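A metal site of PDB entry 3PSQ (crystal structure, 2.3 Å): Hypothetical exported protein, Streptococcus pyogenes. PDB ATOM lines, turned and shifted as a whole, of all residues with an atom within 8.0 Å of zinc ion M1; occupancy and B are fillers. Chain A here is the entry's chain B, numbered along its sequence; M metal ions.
OE2 of Glu 55 binds zinc ion M1, at 1.8 Å.
OD2 of Asp 35 is bound to zinc ion M1 (2.0 Å).
Zinc ion M1 is bound by OE2 of Glu 59, 2.2 Å away.
Zinc ion M1 has three donor atoms within binding distance.
Slightly farther from zinc ion M1 lies OE1 of Glu 59 (2.7 Å).
Slightly farther from zinc ion M1 lies OE1 of Glu 55 (2.8 Å).
OD2 of Asp 35 sits close to OH of Tyr 60 (2.6 Å).
O of Asp 35 is in hydrogen-bond range of N of Gln 53, 2.9 Å away.
N of Asp 35 sits at hydrogen-bond distance from OD1 of Asn 33, 2.7 Å away.
The side-chain amino group (NZ) of Lys 63 sits close to the side-chain carboxylate (OE2) of Glu 59 (2.7 Å).
The side-chain amide oxygen (OD1) of Asn 56 is in hydrogen-bond range of the backbone NH (N) of Glu 59.
Three residues have an atom within 4 Å of zinc ion M1: Asp 35, Glu 55 and Glu 59.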
ATOM      1  N   ASN A  33     -25.855   8.978  -7.563  1.00  0.00           N
ATOM      2  CA  ASN A  33     -25.504   9.823  -6.423  1.00  0.00           C
ATOM      3  C   ASN A  33     -26.368  11.076  -6.407  1.00  0.00           C
ATOM      4  O   ASN A  33     -26.237  11.952  -7.250  1.00  0.00           O
ATOM      5  CB  ASN A  33     -24.012  10.166  -6.490  1.00  0.00           C
ATOM      6  CG  ASN A  33     -23.526  10.988  -5.300  1.00  0.00           C
ATOM      7  OD1 ASN A  33     -24.301  11.511  -4.510  1.00  0.00           O
ATOM      8  ND2 ASN A  33     -22.205  11.089  -5.181  1.00  0.00           N
ATOM      9  N   SER A  34     -27.241  11.149  -5.416  1.00  0.00           N
ATOM     10  CA  SER A  34     -28.116  12.280  -5.273  1.00  0.00           C
ATOM     11  C   SER A  34     -27.376  13.616  -5.048  1.00  0.00           C
ATOM     12  O   SER A  34     -27.989  14.678  -5.176  1.00  0.00           O
ATOM     13  CB  SER A  34     -29.117  11.997  -4.149  1.00  0.00           C
ATOM     14  OG  SER A  34     -28.479  11.911  -2.878  1.00  0.00           O
ATOM     15  N   ASP A  35     -26.075  13.557  -4.710  1.00  0.00           N
ATOM     16  CA  ASP A  35     -25.267  14.772  -4.399  1.00  0.00           C
ATOM     17  C   ASP A  35     -24.681  15.422  -5.678  1.00  0.00           C
ATOM     18  O   ASP A  35     -24.259  16.591  -5.666  1.00  0.00           O
ATOM     19  CB  ASP A  35     -24.118  14.461  -3.443  1.00  0.00           C
ATOM     20  CG  ASP A  35     -24.557  14.205  -1.988  1.00  0.00           C
ATOM     21  OD1 ASP A  35     -25.711  14.572  -1.615  1.00  0.00           O
ATOM     22  OD2 ASP A  35     -23.692  13.659  -1.195  1.00  0.00           O
ATOM     23  N   VAL A  36     -24.657  14.658  -6.781  1.00  0.00           N
ATOM     24  CA  VAL A  36     -24.322  15.204  -8.098  1.00  0.00           C
ATOM     25  C   VAL A  36     -25.250  16.350  -8.536  1.00  0.00           C
ATOM     26  O   VAL A  36     -26.485  16.208  -8.505  1.00  0.00           O
ATOM     27  CB  VAL A  36     -24.331  14.135  -9.161  1.00  0.00           C
ATOM     28  CG1 VAL A  36     -23.954  14.738 -10.534  1.00  0.00           C
ATOM     29  CG2 VAL A  36     -23.333  13.088  -8.774  1.00  0.00           C
ATOM     30  N   VAL A  52     -20.166  17.593  -7.288  1.00  0.00           N
ATOM     31  CA  VAL A  52     -21.166  17.239  -6.275  1.00  0.00           C
ATOM     32  C   VAL A  52     -21.237  18.355  -5.293  1.00  0.00           C
ATOM     33  O   VAL A  52     -20.396  19.211  -5.291  1.00  0.00           O
ATOM     34  CB  VAL A  52     -20.802  15.938  -5.486  1.00  0.00           C
ATOM     35  CG1 VAL A  52     -20.832  14.722  -6.389  1.00  0.00           C
ATOM     36  CG2 VAL A  52     -19.412  16.106  -4.795  1.00  0.00           C
ATOM     37  N   GLN A  53     -22.272  18.356  -4.479  1.00  0.00           N
ATOM     38  CA  GLN A  53     -22.306  19.189  -3.314  1.00  0.00           C
ATOM     39  C   GLN A  53     -22.659  18.308  -2.097  1.00  0.00           C
ATOM     40  O   GLN A  53     -23.652  17.559  -2.110  1.00  0.00           O
ATOM     41  CB  GLN A  53     -23.333  20.305  -3.451  1.00  0.00           C
ATOM     42  CG  GLN A  53     -23.159  21.358  -2.396  1.00  0.00           C
ATOM     43  CD  GLN A  53     -24.318  22.305  -2.254  1.00  0.00           C
ATOM     44  OE1 GLN A  53     -25.483  21.902  -2.281  1.00  0.00           O
ATOM     45  NE2 GLN A  53     -24.006  23.578  -2.016  1.00  0.00           N
ATOM     46  N   GLY A  54     -21.809  18.373  -1.059  1.00  0.00           N
ATOM     47  CA  GLY A  54     -21.987  17.532   0.121  1.00  0.00           C
ATOM     48  C   GLY A  54     -22.749  18.323   1.123  1.00  0.00           C
ATOM     49  O   GLY A  54     -23.054  19.522   0.918  1.00  0.00           O
ATOM     50  N   GLU A  55     -23.090  17.694   2.252  1.00  0.00           N
ATOM     51  CA  GLU A  55     -23.860  18.406   3.275  1.00  0.00           C
ATOM     52  C   GLU A  55     -22.922  19.275   4.099  1.00  0.00           C
ATOM     53  O   GLU A  55     -23.346  20.109   4.893  1.00  0.00           O
ATOM     54  CB  GLU A  55     -24.688  17.424   4.101  1.00  0.00           C
ATOM     55  CG  GLU A  55     -25.632  16.531   3.257  1.00  0.00           C
ATOM     56  CD  GLU A  55     -24.968  15.306   2.681  1.00  0.00           C
ATOM     57  OE1 GLU A  55     -24.471  14.486   3.469  1.00  0.00           O
ATOM     58  OE2 GLU A  55     -24.930  15.126   1.443  1.00  0.00           O
ATOM     59  N   ASN A  56     -21.619  19.137   3.837  1.00  0.00           N
ATOM     60  CA  ASN A  56     -20.588  19.915   4.512  1.00  0.00           C
ATOM     61  C   ASN A  56     -19.369  19.838   3.610  1.00  0.00           C
ATOM     62  O   ASN A  56     -19.400  19.125   2.620  1.00  0.00           O
ATOM     63  CB  ASN A  56     -20.259  19.272   5.886  1.00  0.00           C
ATOM     64  CG  ASN A  56     -19.997  17.781   5.748  1.00  0.00           C
ATOM     65  OD1 ASN A  56     -18.894  17.367   5.324  1.00  0.00           O
ATOM     66  ND2 ASN A  56     -21.011  16.954   6.042  1.00  0.00           N
ATOM     67  N   GLU A  59     -17.242  16.026   3.448  1.00  0.00           N
ATOM     68  CA  GLU A  59     -17.827  14.799   2.887  1.00  0.00           C
ATOM     69  C   GLU A  59     -17.051  14.208   1.675  1.00  0.00           C
ATOM     70  O   GLU A  59     -16.877  12.987   1.552  1.00  0.00           O
ATOM     71  CB  GLU A  59     -19.303  15.096   2.503  1.00  0.00           C
ATOM     72  CG  GLU A  59     -19.919  13.928   1.826  1.00  0.00           C
ATOM     73  CD  GLU A  59     -21.408  14.055   1.581  1.00  0.00           C
ATOM     74  OE1 GLU A  59     -21.975  15.168   1.763  1.00  0.00           O
ATOM     75  OE2 GLU A  59     -21.997  13.028   1.184  1.00  0.00           O
ATOM     76  N   TYR A  60     -16.568  15.088   0.790  1.00  0.00           N
ATOM     77  CA  TYR A  60     -15.967  14.640  -0.460  1.00  0.00           C
ATOM     78  C   TYR A  60     -14.446  14.794  -0.563  1.00  0.00           C
ATOM     79  O   TYR A  60     -13.889  14.673  -1.667  1.00  0.00           O
ATOM     80  CB  TYR A  60     -16.728  15.265  -1.653  1.00  0.00           C
ATOM     81  CG  TYR A  60     -18.101  14.614  -1.848  1.00  0.00           C
ATOM     82  CD1 TYR A  60     -18.167  13.357  -2.408  1.00  0.00           C
ATOM     83  CD2 TYR A  60     -19.294  15.250  -1.474  1.00  0.00           C
ATOM     84  CE1 TYR A  60     -19.343  12.721  -2.598  1.00  0.00           C
ATOM     85  CE2 TYR A  60     -20.565  14.592  -1.681  1.00  0.00           C
ATOM     86  CZ  TYR A  60     -20.542  13.321  -2.221  1.00  0.00           C
ATOM     87  OH  TYR A  60     -21.656  12.545  -2.446  1.00  0.00           O
ATOM     88  N   LYS A  63     -13.987  10.747  -0.668  1.00  0.00           N
ATOM     89  CA  LYS A  63     -15.097   9.956  -1.207  1.00  0.00           C
ATOM     90  C   LYS A  63     -15.325  10.309  -2.667  1.00  0.00           C
ATOM     91  O   LYS A  63     -15.419  11.486  -3.051  1.00  0.00           O
ATOM     92  CB  LYS A  63     -16.383  10.208  -0.393  1.00  0.00           C
ATOM     93  CG  LYS A  63     -17.578   9.385  -0.842  1.00  0.00           C
ATOM     94  CD  LYS A  63     -18.727   9.371   0.150  1.00  0.00           C
ATOM     95  CE  LYS A  63     -19.341  10.775   0.355  1.00  0.00           C
ATOM     96  NZ  LYS A  63     -20.665  10.728   1.117  1.00  0.00           N
HETATM   97 ZN    ZN M   1     -24.069  13.680   0.786  1.00  0.00          ZN
HETATM   98 ZN    ZN M   2     -27.372  18.444  -0.621  1.00  0.00          ZN
